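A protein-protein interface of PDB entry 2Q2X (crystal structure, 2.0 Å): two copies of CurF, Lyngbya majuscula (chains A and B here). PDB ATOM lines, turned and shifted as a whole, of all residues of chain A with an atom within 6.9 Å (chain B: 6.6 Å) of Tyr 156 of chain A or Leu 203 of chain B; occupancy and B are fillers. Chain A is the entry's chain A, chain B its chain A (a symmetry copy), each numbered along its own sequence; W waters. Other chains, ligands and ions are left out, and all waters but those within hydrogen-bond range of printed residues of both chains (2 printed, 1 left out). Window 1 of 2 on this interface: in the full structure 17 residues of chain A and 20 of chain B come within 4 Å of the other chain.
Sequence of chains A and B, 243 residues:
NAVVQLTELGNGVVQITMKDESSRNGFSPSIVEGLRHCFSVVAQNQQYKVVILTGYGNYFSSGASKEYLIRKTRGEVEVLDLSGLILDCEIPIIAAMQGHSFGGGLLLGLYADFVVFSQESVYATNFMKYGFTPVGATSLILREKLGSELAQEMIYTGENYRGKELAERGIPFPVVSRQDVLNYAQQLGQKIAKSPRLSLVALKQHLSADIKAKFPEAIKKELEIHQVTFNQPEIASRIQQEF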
ATOM      1  N   THR A 125     -35.057  20.186 -30.837  1.00  0.00           N
ATOM      2  CA  THR A 125     -33.997  21.037 -31.378  1.00  0.00           C
ATOM      3  C   THR A 125     -33.250  20.141 -32.345  1.00  0.00           C
ATOM      4  O   THR A 125     -32.342  19.409 -31.936  1.00  0.00           O
ATOM      5  CB  THR A 125     -33.023  21.630 -30.302  1.00  0.00           C
ATOM      6  OG1 THR A 125     -32.594  20.610 -29.400  1.00  0.00           O
ATOM      7  CG2 THR A 125     -33.712  22.712 -29.524  1.00  0.00           C
ATOM      8  N   MET A 128     -28.735  18.785 -34.539  1.00  0.00           N
ATOM      9  CA  MET A 128     -27.860  17.628 -34.483  1.00  0.00           C
ATOM     10  C   MET A 128     -28.460  16.359 -35.091  1.00  0.00           C
ATOM     11  O   MET A 128     -27.748  15.404 -35.322  1.00  0.00           O
ATOM     12  CB  MET A 128     -27.346  17.379 -33.065  1.00  0.00           C
ATOM     13  CG  MET A 128     -26.328  18.419 -32.593  1.00  0.00           C
ATOM     14  SD  MET A 128     -24.574  18.247 -33.470  1.00  0.00           S
ATOM     15  CE  MET A 128     -23.808  16.890 -32.345  1.00  0.00           C
ATOM     16  N   LYS A 129     -29.757  16.348 -35.365  1.00  0.00           N
ATOM     17  CA  LYS A 129     -30.322  15.237 -36.140  1.00  0.00           C
ATOM     18  C   LYS A 129     -29.615  15.191 -37.511  1.00  0.00           C
ATOM     19  O   LYS A 129     -29.300  14.113 -38.017  1.00  0.00           O
ATOM     20  CB  LYS A 129     -31.829  15.403 -36.326  1.00  0.00           C
ATOM     21  CG  LYS A 129     -32.538  14.147 -36.808  1.00  0.00           C
ATOM     22  CD  LYS A 129     -33.993  14.441 -37.160  1.00  0.00           C
ATOM     23  CE  LYS A 129     -34.793  13.142 -37.319  1.00  0.00           C
ATOM     24  NZ  LYS A 129     -36.277  13.343 -37.294  1.00  0.00           N
ATOM     25  N   PHE A 132     -25.189  18.764 -37.363  1.00  0.00           N
ATOM     26  CA  PHE A 132     -24.569  20.072 -37.116  1.00  0.00           C
ATOM     27  C   PHE A 132     -25.125  20.790 -35.878  1.00  0.00           C
ATOM     28  O   PHE A 132     -26.205  20.455 -35.385  1.00  0.00           O
ATOM     29  CB  PHE A 132     -24.621  20.995 -38.351  1.00  0.00           C
ATOM     30  CG  PHE A 132     -26.006  21.274 -38.857  1.00  0.00           C
ATOM     31  CD1 PHE A 132     -26.797  22.270 -38.269  1.00  0.00           C
ATOM     32  CD2 PHE A 132     -26.530  20.539 -39.923  1.00  0.00           C
ATOM     33  CE1 PHE A 132     -28.097  22.522 -38.733  1.00  0.00           C
ATOM     34  CE2 PHE A 132     -27.813  20.790 -40.383  1.00  0.00           C
ATOM     35  CZ  PHE A 132     -28.589  21.786 -39.804  1.00  0.00           C
ATOM     36  N   THR A 133     -24.394  21.814 -35.442  1.00  0.00           N
ATOM     37  CA  THR A 133     -24.717  22.589 -34.234  1.00  0.00           C
ATOM     38  C   THR A 133     -25.787  23.672 -34.398  1.00  0.00           C
ATOM     39  O   THR A 133     -26.042  24.154 -35.514  1.00  0.00           O
ATOM     40  CB  THR A 133     -23.416  23.131 -33.564  1.00  0.00           C
ATOM     41  OG1 THR A 133     -22.742  24.047 -34.439  1.00  0.00           O
ATOM     42  CG2 THR A 133     -22.490  21.989 -33.249  1.00  0.00           C
ATOM     43  N   PRO A 134     -26.452  24.051 -33.279  1.00  0.00           N
ATOM     44  CA  PRO A 134     -27.588  24.975 -33.318  1.00  0.00           C
ATOM     45  C   PRO A 134     -27.235  26.388 -33.731  1.00  0.00           C
ATOM     46  O   PRO A 134     -26.075  26.772 -33.694  1.00  0.00           O
ATOM     47  CB  PRO A 134     -28.071  25.023 -31.844  1.00  0.00           C
ATOM     48  CG  PRO A 134     -27.462  23.874 -31.174  1.00  0.00           C
ATOM     49  CD  PRO A 134     -26.172  23.588 -31.903  1.00  0.00           C
ATOM     50  N   SER A 139     -28.445  26.999 -26.916  1.00  0.00           N
ATOM     51  CA  SER A 139     -27.819  26.627 -25.638  1.00  0.00           C
ATOM     52  C   SER A 139     -28.284  27.553 -24.498  1.00  0.00           C
ATOM     53  O   SER A 139     -28.732  27.088 -23.448  1.00  0.00           O
ATOM     54  CB  SER A 139     -26.302  26.698 -25.785  1.00  0.00           C
ATOM     55  OG  SER A 139     -25.647  26.372 -24.577  1.00  0.00           O
ATOM     56  N   ALA A 151     -31.800  20.173 -21.626  1.00  0.00           N
ATOM     57  CA  ALA A 151     -31.298  20.967 -22.753  1.00  0.00           C
ATOM     58  C   ALA A 151     -30.157  20.245 -23.459  1.00  0.00           C
ATOM     59  O   ALA A 151     -30.176  20.107 -24.671  1.00  0.00           O
ATOM     60  CB  ALA A 151     -30.845  22.336 -22.290  1.00  0.00           C
ATOM     61  N   GLN A 152     -29.181  19.788 -22.681  1.00  0.00           N
ATOM     62  CA  GLN A 152     -28.013  19.086 -23.182  1.00  0.00           C
ATOM     63  C   GLN A 152     -28.386  17.832 -23.989  1.00  0.00           C
ATOM     64  O   GLN A 152     -27.901  17.637 -25.111  1.00  0.00           O
ATOM     65  CB  GLN A 152     -27.086  18.747 -22.025  1.00  0.00           C
ATOM     66  CG  GLN A 152     -25.767  18.063 -22.402  1.00  0.00           C
ATOM     67  CD  GLN A 152     -24.559  18.694 -21.704  1.00  0.00           C
ATOM     68  OE1 GLN A 152     -24.541  19.898 -21.435  1.00  0.00           O
ATOM     69  NE2 GLN A 152     -23.554  17.886 -21.412  1.00  0.00           N
ATOM     70  N   GLU A 153     -29.273  17.012 -23.439  1.00  0.00           N
ATOM     71  CA  GLU A 153     -29.718  15.820 -24.156  1.00  0.00           C
ATOM     72  C   GLU A 153     -30.468  16.166 -25.439  1.00  0.00           C
ATOM     73  O   GLU A 153     -30.202  15.579 -26.500  1.00  0.00           O
ATOM     74  CB  GLU A 153     -30.571  14.922 -23.254  1.00  0.00           C
ATOM     75  CG  GLU A 153     -30.936  13.596 -23.895  1.00  0.00           C
ATOM     76  CD  GLU A 153     -31.949  12.822 -23.087  1.00  0.00           C
ATOM     77  OE1 GLU A 153     -31.592  12.374 -21.978  1.00  0.00           O
ATOM     78  OE2 GLU A 153     -33.095  12.663 -23.568  1.00  0.00           O
ATOM     79  N   MET A 154     -31.393  17.121 -25.353  1.00  0.00           N
ATOM     80  CA  MET A 154     -32.140  17.568 -26.523  1.00  0.00           C
ATOM     81  C   MET A 154     -31.223  18.150 -27.594  1.00  0.00           C
ATOM     82  O   MET A 154     -31.476  17.949 -28.792  1.00  0.00           O
ATOM     83  CB  MET A 154     -33.194  18.604 -26.149  1.00  0.00           C
ATOM     84  CG  MET A 154     -34.344  18.044 -25.329  1.00  0.00           C
ATOM     85  SD  MET A 154     -35.721  19.391 -25.113  1.00  0.00           S
ATOM     86  CE  MET A 154     -36.564  19.300 -26.871  1.00  0.00           C
ATOM     87  N   ILE A 155     -30.162  18.842 -27.171  1.00  0.00           N
ATOM     88  CA  ILE A 155     -29.245  19.483 -28.138  1.00  0.00           C
ATOM     89  C   ILE A 155     -28.289  18.464 -28.795  1.00  0.00           C
ATOM     90  O   ILE A 155     -28.151  18.450 -30.014  1.00  0.00           O
ATOM     91  CB  ILE A 155     -28.457  20.687 -27.544  1.00  0.00           C
ATOM     92  CG1 ILE A 155     -29.415  21.812 -27.144  1.00  0.00           C
ATOM     93  CG2 ILE A 155     -27.466  21.244 -28.609  1.00  0.00           C
ATOM     94  CD1 ILE A 155     -28.808  22.867 -26.192  1.00  0.00           C
ATOM     95  N   TYR A 156     -27.648  17.624 -27.987  1.00  0.00           N
ATOM     96  CA  TYR A 156     -26.759  16.580 -28.503  1.00  0.00           C
ATOM     97  C   TYR A 156     -27.451  15.633 -29.477  1.00  0.00           C
ATOM     98  O   TYR A 156     -26.875  15.280 -30.502  1.00  0.00           O
ATOM     99  CB  TYR A 156     -26.156  15.760 -27.372  1.00  0.00           C
ATOM    100  CG  TYR A 156     -24.816  16.221 -26.859  1.00  0.00           C
ATOM    101  CD1 TYR A 156     -23.622  15.748 -27.426  1.00  0.00           C
ATOM    102  CD2 TYR A 156     -24.733  17.102 -25.792  1.00  0.00           C
ATOM    103  CE1 TYR A 156     -22.382  16.160 -26.936  1.00  0.00           C
ATOM    104  CE2 TYR A 156     -23.510  17.516 -25.296  1.00  0.00           C
ATOM    105  CZ  TYR A 156     -22.339  17.048 -25.866  1.00  0.00           C
ATOM    106  OH  TYR A 156     -21.134  17.473 -25.339  1.00  0.00           O
ATOM    107  N   THR A 157     -28.680  15.217 -29.162  1.00  0.00           N
ATOM    108  CA  THR A 157     -29.342  14.167 -29.954  1.00  0.00           C
ATOM    109  C   THR A 157     -30.129  14.693 -31.150  1.00  0.00           C
ATOM    110  O   THR A 157     -30.185  14.035 -32.190  1.00  0.00           O
ATOM    111  CB  THR A 157     -30.275  13.276 -29.106  1.00  0.00           C
ATOM    112  OG1 THR A 157     -31.417  14.035 -28.695  1.00  0.00           O
ATOM    113  CG2 THR A 157     -29.550  12.707 -27.903  1.00  0.00           C
ATOM    114  N   GLY A 158     -30.760  15.856 -31.001  1.00  0.00           N
ATOM    115  CA  GLY A 158     -31.617  16.420 -32.037  1.00  0.00           C
ATOM    116  C   GLY A 158     -32.955  15.702 -32.117  1.00  0.00           C
ATOM    117  O   GLY A 158     -33.809  16.015 -32.966  1.00  0.00           O
ATOM    118  N   GLU A 159     -33.152  14.746 -31.219  1.00  0.00           N
ATOM    119  CA  GLU A 159     -34.312  13.857 -31.291  1.00  0.00           C
ATOM    120  C   GLU A 159     -35.640  14.494 -30.909  1.00  0.00           C
ATOM    121  O   GLU A 159     -35.679  15.580 -30.303  1.00  0.00           O
ATOM    122  CB  GLU A 159     -34.055  12.604 -30.469  1.00  0.00           C
ATOM    123  CG  GLU A 159     -33.064  11.669 -31.115  1.00  0.00           C
ATOM    124  CD  GLU A 159     -32.965  10.334 -30.397  1.00  0.00           C
ATOM    125  OE1 GLU A 159     -32.438   9.376 -31.005  1.00  0.00           O
ATOM    126  OE2 GLU A 159     -33.417  10.240 -29.234  1.00  0.00           O
ATOM    127  N   GLU A 222     -22.604  30.891 -31.296  1.00  0.00           N
ATOM    128  CA  GLU A 222     -23.253  29.722 -31.869  1.00  0.00           C
ATOM    129  C   GLU A 222     -23.175  29.716 -33.385  1.00  0.00           C
ATOM    130  O   GLU A 222     -22.984  28.672 -34.004  1.00  0.00           O
ATOM    131  CB  GLU A 222     -24.711  29.639 -31.429  1.00  0.00           C
ATOM    132  CG  GLU A 222     -24.927  28.457 -30.565  1.00  0.00           C
ATOM    133  CD  GLU A 222     -26.323  28.336 -30.010  1.00  0.00           C
ATOM    134  OE1 GLU A 222     -27.298  28.736 -30.704  1.00  0.00           O
ATOM    135  OE2 GLU A 222     -26.416  27.781 -28.882  1.00  0.00           O
ATOM    136  N   ILE A 225     -19.755  28.614 -34.646  1.00  0.00           N
ATOM    137  CA  ILE A 225     -19.611  27.163 -34.556  1.00  0.00           C
ATOM    138  C   ILE A 225     -20.500  26.465 -35.588  1.00  0.00           C
ATOM    139  O   ILE A 225     -20.069  25.491 -36.220  1.00  0.00           O
ATOM    140  CB  ILE A 225     -19.911  26.669 -33.120  1.00  0.00           C
ATOM    141  CG1 ILE A 225     -18.948  27.340 -32.145  1.00  0.00           C
ATOM    142  CG2 ILE A 225     -19.783  25.139 -33.013  1.00  0.00           C
ATOM    143  CD1 ILE A 225     -19.552  27.525 -30.737  1.00  0.00           C
ATOM    144  N   THR A 229     -19.608  23.600 -38.473  1.00  0.00           N
ATOM    145  CA  THR A 229     -20.089  22.226 -38.414  1.00  0.00           C
ATOM    146  C   THR A 229     -21.093  21.936 -39.529  1.00  0.00           C
ATOM    147  O   THR A 229     -21.205  20.793 -39.962  1.00  0.00           O
ATOM    148  CB  THR A 229     -20.722  21.866 -37.026  1.00  0.00           C
ATOM    149  OG1 THR A 229     -21.799  22.750 -36.768  1.00  0.00           O
ATOM    150  CG2 THR A 229     -19.706  22.012 -35.887  1.00  0.00           C
ATOM    151  N   ILE B  91     -13.956  14.870 -26.046  1.00  0.00           N
ATOM    152  CA  ILE B  91     -15.195  14.206 -26.441  1.00  0.00           C
ATOM    153  C   ILE B  91     -16.141  13.966 -25.254  1.00  0.00           C
ATOM    154  O   ILE B  91     -15.678  13.873 -24.120  1.00  0.00           O
ATOM    155  CB  ILE B  91     -14.908  12.887 -27.200  1.00  0.00           C
ATOM    156  CG1 ILE B  91     -14.125  11.889 -26.328  1.00  0.00           C
ATOM    157  CG2 ILE B  91     -14.181  13.192 -28.518  1.00  0.00           C
ATOM    158  CD1 ILE B  91     -13.992  10.463 -26.937  1.00  0.00           C
ATOM    159  N   PRO B  92     -17.471  13.890 -25.510  1.00  0.00           N
ATOM    160  CA  PRO B  92     -18.412  13.676 -24.408  1.00  0.00           C
ATOM    161  C   PRO B  92     -18.109  12.415 -23.617  1.00  0.00           C
ATOM    162  O   PRO B  92     -17.688  11.389 -24.191  1.00  0.00           O
ATOM    163  CB  PRO B  92     -19.780  13.575 -25.104  1.00  0.00           C
ATOM    164  CG  PRO B  92     -19.477  13.389 -26.551  1.00  0.00           C
ATOM    165  CD  PRO B  92     -18.173  14.070 -26.795  1.00  0.00           C
ATOM    166  N   ILE B  93     -18.277  12.524 -22.301  1.00  0.00           N
ATOM    167  CA  ILE B  93     -18.071  11.424 -21.379  1.00  0.00           C
ATOM    168  C   ILE B  93     -19.412  11.174 -20.724  1.00  0.00           C
ATOM    169  O   ILE B  93     -20.116  12.115 -20.338  1.00  0.00           O
ATOM    170  CB  ILE B  93     -17.015  11.771 -20.267  1.00  0.00           C
ATOM    171  CG1 ILE B  93     -15.646  12.083 -20.878  1.00  0.00           C
ATOM    172  CG2 ILE B  93     -16.876  10.633 -19.250  1.00  0.00           C
ATOM    173  CD1 ILE B  93     -14.744  12.899 -19.957  1.00  0.00           C
ATOM    174  N   ASP B 113     -20.244  14.872 -18.955  1.00  0.00           N
ATOM    175  CA  ASP B 113     -21.288  15.570 -19.705  1.00  0.00           C
ATOM    176  C   ASP B 113     -22.661  14.953 -19.461  1.00  0.00           C
ATOM    177  O   ASP B 113     -23.667  15.653 -19.440  1.00  0.00           O
ATOM    178  CB  ASP B 113     -20.932  15.555 -21.181  1.00  0.00           C
ATOM    179  CG  ASP B 113     -19.535  16.066 -21.421  1.00  0.00           C
ATOM    180  OD1 ASP B 113     -19.356  17.290 -21.351  1.00  0.00           O
ATOM    181  OD2 ASP B 113     -18.607  15.244 -21.626  1.00  0.00           O
ATOM    182  N   PHE B 114     -22.677  13.641 -19.264  1.00  0.00           N
ATOM    183  CA  PHE B 114     -23.898  12.919 -18.925  1.00  0.00           C
ATOM    184  C   PHE B 114     -23.576  12.029 -17.724  1.00  0.00           C
ATOM    185  O   PHE B 114     -22.446  11.522 -17.611  1.00  0.00           O
ATOM    186  CB  PHE B 114     -24.352  12.060 -20.108  1.00  0.00           C
ATOM    187  CG  PHE B 114     -24.669  12.860 -21.343  1.00  0.00           C
ATOM    188  CD1 PHE B 114     -23.666  13.174 -22.263  1.00  0.00           C
ATOM    189  CD2 PHE B 114     -25.966  13.318 -21.576  1.00  0.00           C
ATOM    190  CE1 PHE B 114     -23.946  13.930 -23.388  1.00  0.00           C
ATOM    191  CE2 PHE B 114     -26.256  14.080 -22.703  1.00  0.00           C
ATOM    192  CZ  PHE B 114     -25.253  14.390 -23.605  1.00  0.00           C
ATOM    193  N   LYS B 191     -26.189   6.444 -29.382  1.00  0.00           N
ATOM    194  CA  LYS B 191     -27.084   7.509 -29.834  1.00  0.00           C
ATOM    195  C   LYS B 191     -26.273   8.767 -30.200  1.00  0.00           C
ATOM    196  O   LYS B 191     -26.343   9.259 -31.327  1.00  0.00           O
ATOM    197  CB  LYS B 191     -28.123   7.813 -28.749  1.00  0.00           C
ATOM    198  CG  LYS B 191     -29.383   8.495 -29.241  1.00  0.00           C
ATOM    199  CD  LYS B 191     -30.636   7.757 -28.750  1.00  0.00           C
ATOM    200  CE  LYS B 191     -31.275   8.427 -27.546  1.00  0.00           C
ATOM    201  NZ  LYS B 191     -32.554   7.750 -27.151  1.00  0.00           N
ATOM    202  N   ILE B 192     -25.477   9.248 -29.249  1.00  0.00           N
ATOM    203  CA  ILE B 192     -24.614  10.416 -29.439  1.00  0.00           C
ATOM    204  C   ILE B 192     -23.605  10.203 -30.560  1.00  0.00           C
ATOM    205  O   ILE B 192     -23.380  11.108 -31.379  1.00  0.00           O
ATOM    206  CB  ILE B 192     -23.892  10.777 -28.118  1.00  0.00           C
ATOM    207  CG1 ILE B 192     -24.923  11.117 -27.042  1.00  0.00           C
ATOM    208  CG2 ILE B 192     -22.917  11.934 -28.316  1.00  0.00           C
ATOM    209  CD1 ILE B 192     -24.363  11.090 -25.613  1.00  0.00           C
ATOM    210  N   SER B 195     -23.498  11.250 -34.474  1.00  0.00           N
ATOM    211  CA  SER B 195     -23.070  12.559 -34.959  1.00  0.00           C
ATOM    212  C   SER B 195     -21.620  12.594 -35.426  1.00  0.00           C
ATOM    213  O   SER B 195     -20.808  11.823 -34.933  1.00  0.00           O
ATOM    214  CB  SER B 195     -23.247  13.605 -33.860  1.00  0.00           C
ATOM    215  OG  SER B 195     -24.612  13.792 -33.538  1.00  0.00           O
ATOM    216  N   LEU B 198     -16.412  15.881 -35.230  1.00  0.00           N
ATOM    217  CA  LEU B 198     -16.127  17.313 -35.211  1.00  0.00           C
ATOM    218  C   LEU B 198     -17.243  18.139 -34.558  1.00  0.00           C
ATOM    219  O   LEU B 198     -16.974  19.130 -33.863  1.00  0.00           O
ATOM    220  CB  LEU B 198     -15.914  17.798 -36.644  1.00  0.00           C
ATOM    221  CG  LEU B 198     -15.479  19.233 -36.942  1.00  0.00           C
ATOM    222  CD1 LEU B 198     -14.681  19.220 -38.234  1.00  0.00           C
ATOM    223  CD2 LEU B 198     -16.663  20.164 -37.093  1.00  0.00           C
ATOM    224  N   SER B 199     -18.493  17.756 -34.828  1.00  0.00           N
ATOM    225  CA  SER B 199     -19.650  18.452 -34.276  1.00  0.00           C
ATOM    226  C   SER B 199     -19.744  18.182 -32.769  1.00  0.00           C
ATOM    227  O   SER B 199     -20.084  19.080 -31.999  1.00  0.00           O
ATOM    228  CB  SER B 199     -20.936  17.995 -34.964  1.00  0.00           C
ATOM    229  OG  SER B 199     -21.045  18.503 -36.289  1.00  0.00           O
ATOM    230  N   LEU B 200     -19.458  16.941 -32.379  1.00  0.00           N
ATOM    231  CA  LEU B 200     -19.456  16.505 -30.979  1.00  0.00           C
ATOM    232  C   LEU B 200     -18.404  17.248 -30.158  1.00  0.00           C
ATOM    233  O   LEU B 200     -18.678  17.695 -29.026  1.00  0.00           O
ATOM    234  CB  LEU B 200     -19.228  14.991 -30.888  1.00  0.00           C
ATOM    235  CG  LEU B 200     -20.401  14.076 -31.273  1.00  0.00           C
ATOM    236  CD1 LEU B 200     -20.012  12.624 -31.108  1.00  0.00           C
ATOM    237  CD2 LEU B 200     -21.640  14.377 -30.426  1.00  0.00           C
ATOM    238  N   VAL B 201     -17.210  17.391 -30.738  1.00  0.00           N
ATOM    239  CA  VAL B 201     -16.118  18.123 -30.101  1.00  0.00           C
ATOM    240  C   VAL B 201     -16.466  19.612 -29.992  1.00  0.00           C
ATOM    241  O   VAL B 201     -16.297  20.220 -28.927  1.00  0.00           O
ATOM    242  CB  VAL B 201     -14.750  17.903 -30.847  1.00  0.00           C
ATOM    243  CG1 VAL B 201     -13.649  18.780 -30.260  1.00  0.00           C
ATOM    244  CG2 VAL B 201     -14.323  16.429 -30.804  1.00  0.00           C
ATOM    245  N   ALA B 202     -16.981  20.189 -31.080  1.00  0.00           N
ATOM    246  CA  ALA B 202     -17.355  21.597 -31.102  1.00  0.00           C
ATOM    247  C   ALA B 202     -18.495  21.897 -30.112  1.00  0.00           C
ATOM    248  O   ALA B 202     -18.466  22.902 -29.368  1.00  0.00           O
ATOM    249  CB  ALA B 202     -17.747  22.013 -32.520  1.00  0.00           C
ATOM    250  N   LEU B 203     -19.502  21.023 -30.109  1.00  0.00           N
ATOM    251  CA  LEU B 203     -20.659  21.219 -29.246  1.00  0.00           C
ATOM    252  C   LEU B 203     -20.257  21.132 -27.779  1.00  0.00           C
ATOM    253  O   LEU B 203     -20.669  21.967 -26.986  1.00  0.00           O
ATOM    254  CB  LEU B 203     -21.768  20.217 -29.590  1.00  0.00           C
ATOM    255  CG  LEU B 203     -23.075  20.339 -28.829  1.00  0.00           C
ATOM    256  CD1 LEU B 203     -23.713  21.732 -29.025  1.00  0.00           C
ATOM    257  CD2 LEU B 203     -24.006  19.204 -29.268  1.00  0.00           C
ATOM    258  N   LYS B 204     -19.424  20.147 -27.432  1.00  0.00           N
ATOM    259  CA  LYS B 204     -18.979  19.969 -26.057  1.00  0.00           C
ATOM    260  C   LYS B 204     -18.251  21.217 -25.554  1.00  0.00           C
ATOM    261  O   LYS B 204     -18.531  21.702 -24.453  1.00  0.00           O
ATOM    262  CB  LYS B 204     -18.102  18.726 -25.895  1.00  0.00           C
ATOM    263  CG  LYS B 204     -17.432  18.681 -24.526  1.00  0.00           C
ATOM    264  CD  LYS B 204     -16.927  17.327 -24.140  1.00  0.00           C
ATOM    265  CE  LYS B 204     -16.241  17.418 -22.782  1.00  0.00           C
ATOM    266  NZ  LYS B 204     -16.041  16.083 -22.168  1.00  0.00           N
ATOM    267  N   GLN B 205     -17.341  21.744 -26.366  1.00  0.00           N
ATOM    268  CA  GLN B 205     -16.616  22.950 -26.005  1.00  0.00           C
ATOM    269  C   GLN B 205     -17.569  24.113 -25.761  1.00  0.00           C
ATOM    270  O   GLN B 205     -17.404  24.865 -24.808  1.00  0.00           O
ATOM    271  CB  GLN B 205     -15.564  23.289 -27.073  1.00  0.00           C
ATOM    272  CG  GLN B 205     -14.773  24.568 -26.797  1.00  0.00           C
ATOM    273  CD  GLN B 205     -13.482  24.625 -27.577  1.00  0.00           C
ATOM    274  OE1 GLN B 205     -12.401  24.696 -26.992  1.00  0.00           O
ATOM    275  NE2 GLN B 205     -13.581  24.575 -28.901  1.00  0.00           N
ATOM    276  N   HIS B 206     -18.594  24.231 -26.607  1.00  0.00           N
ATOM    277  CA  HIS B 206     -19.529  25.344 -26.550  1.00  0.00           C
ATOM    278  C   HIS B 206     -20.364  25.253 -25.288  1.00  0.00           C
ATOM    279  O   HIS B 206     -20.530  26.252 -24.585  1.00  0.00           O
ATOM    280  CB  HIS B 206     -20.436  25.338 -27.799  1.00  0.00           C
ATOM    281  CG  HIS B 206     -21.528  26.356 -27.763  1.00  0.00           C
ATOM    282  ND1 HIS B 206     -21.281  27.712 -27.716  1.00  0.00           N
ATOM    283  CD2 HIS B 206     -22.875  26.218 -27.764  1.00  0.00           C
ATOM    284  CE1 HIS B 206     -22.428  28.365 -27.687  1.00  0.00           C
ATOM    285  NE2 HIS B 206     -23.410  27.481 -27.712  1.00  0.00           N
ATOM    286  N   LEU B 207     -20.874  24.056 -25.002  1.00  0.00           N
ATOM    287  CA  LEU B 207     -21.788  23.853 -23.882  1.00  0.00           C
ATOM    288  C   LEU B 207     -21.063  23.948 -22.552  1.00  0.00           C
ATOM    289  O   LEU B 207     -21.654  24.346 -21.556  1.00  0.00           O
ATOM    290  CB  LEU B 207     -22.521  22.517 -23.999  1.00  0.00           C
ATOM    291  CG  LEU B 207     -23.497  22.322 -25.167  1.00  0.00           C
ATOM    292  CD1 LEU B 207     -24.114  20.930 -25.114  1.00  0.00           C
ATOM    293  CD2 LEU B 207     -24.584  23.377 -25.229  1.00  0.00           C
ATOM    294  N   SER B 208     -19.777  23.619 -22.561  1.00  0.00           N
ATOM    295  CA  SER B 208     -18.908  23.641 -21.372  1.00  0.00           C
ATOM    296  C   SER B 208     -18.283  24.999 -21.022  1.00  0.00           C
ATOM    297  O   SER B 208     -17.675  25.146 -19.955  1.00  0.00           O
ATOM    298  CB  SER B 208     -17.773  22.625 -21.558  1.00  0.00           C
ATOM    299  OG  SER B 208     -18.308  21.315 -21.635  1.00  0.00           O
HETATM  300  O   HOH W   1     -21.227  18.760 -22.886  1.00  0.00           O
HETATM  301  O   HOH W   2     -26.033  13.023 -31.485  1.00  0.00           O
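O of Asp 113 of chain B is in hydrogen-bond range of NE2 of Gln 152 of chain A (3.0 Å). OE2 of Glu 222 of chain A sits at hydrogen-bond distance from NE2 of His 206 of chain B, 3.2 Å away. NZ of Lys 191 of chain B lies within salt-bridge range of OE2 of Glu 159 of chain A (3.4 Å).
Among the printed residues, 25 pairs touch across the chains.
The backbone carbonyl oxygen (O) of Ile 225 of chain A lies within hydrogen-bond range of the side-chain hydroxyl (OG1) of Thr 229 of chain A (3.3 Å). The backbone NH of Ile 93 of chain B lies within hydrogen-bond range of the side-chain carboxylate of Asp 113 of chain B, at 2.8 Å. OG1 of Thr 157 of chain A sits close to N of Glu 159 of chain A, at 3.1 Å. The backbone carbonyl oxygen of Ile 93 of chain B lies within hydrogen-bond range of the backbone NH of Phe 114 of chain B (3.2 Å).
No position is printed for both chains. Of the 25 pairs that touch across the chains among the printed residues, none has its exchanged pair printed and touching as well.
Among the printed residues, pairs that only touch across the chains: Met 128 of chain A with Ser 195 of chain B (3.4 Å), Met 128 of chain A with Ser 199 of chain B (3.9 Å), Met 128 of chain A with Leu 200 of chain B (3.8 Å), Met 128 of chain A with Leu 203 of chain B (3.9 Å), Phe 132 of chain A with Ser 199 of chain B (3.9 Å), Thr 133 of chain A with Ser 199 of chain B (3.98 Å), Ser 139 of chain A with His 206 of chain B (3.6 Å), Ser 139 of chain A with Leu 207 of chain B (3.2 Å), Gln 152 of chain A with Phe 114 of chain B (3.9 Å), Gln 152 of chain A with Leu 207 of chain B (3.8 Å), Ile 155 of chain A with Leu 203 of chain B (3.8 Å), Tyr 156 of chain A with Phe 114 of chain B (3.5 Å), Tyr 156 of chain A with Ile 192 of chain B (3.98 Å), Tyr 156 of chain A with Leu 200 of chain B (3.8 Å), Tyr 156 of chain A with Leu 203 of chain B (3.9 Å), Tyr 156 of chain A with Lys 204 of chain B (3.3 Å), Tyr 156 of chain A with Leu 207 of chain B (3.5 Å), Ile 225 of chain A with Ala 202 of chain B (3.8 Å), Ile 225 of chain A with His 206 of chain B (3.5 Å), Thr 229 of chain A with Leu 198 of chain B (3.8 Å), Thr 229 of chain A with Ser 199 of chain B (3.5 Å) and Thr 229 of chain A with Ala 202 of chain B (3.9 Å).
Water W2 lies within hydrogen-bond range of O of Tyr 156 of chain A, OG of Ser 195 of chain B and O of Ile 192 of chain B. Water W1 lies within hydrogen-bond range of OH of Tyr 156 of chain A (2.8 Å), OD1 of Asp 113 of chain B (2.8 Å) and NE2 of Gln 152 of chain A (2.9 Å).
Tyr 156 of chain A touches just these residues of chain B: Phe 114 (3.5 Å), Ile 192 (3.98 Å), Leu 200 (3.8 Å), Leu 203 (3.9 Å), Lys 204 (3.3 Å) and Leu 207 (3.5 Å). Of the printed residues of chain A, Phe 114 of chain B touches Gln 152 (3.9 Å) and Tyr 156 (3.5 Å). Printed residues of chain A within 4 Å of Leu 200 of chain B: Met 128 and Tyr 156. Leu 203 of chain B touches three residues of chain A. The nearest residue of chain A that does not touch Leu 203 of chain B is Thr 133 of chain A (4.1 Å).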
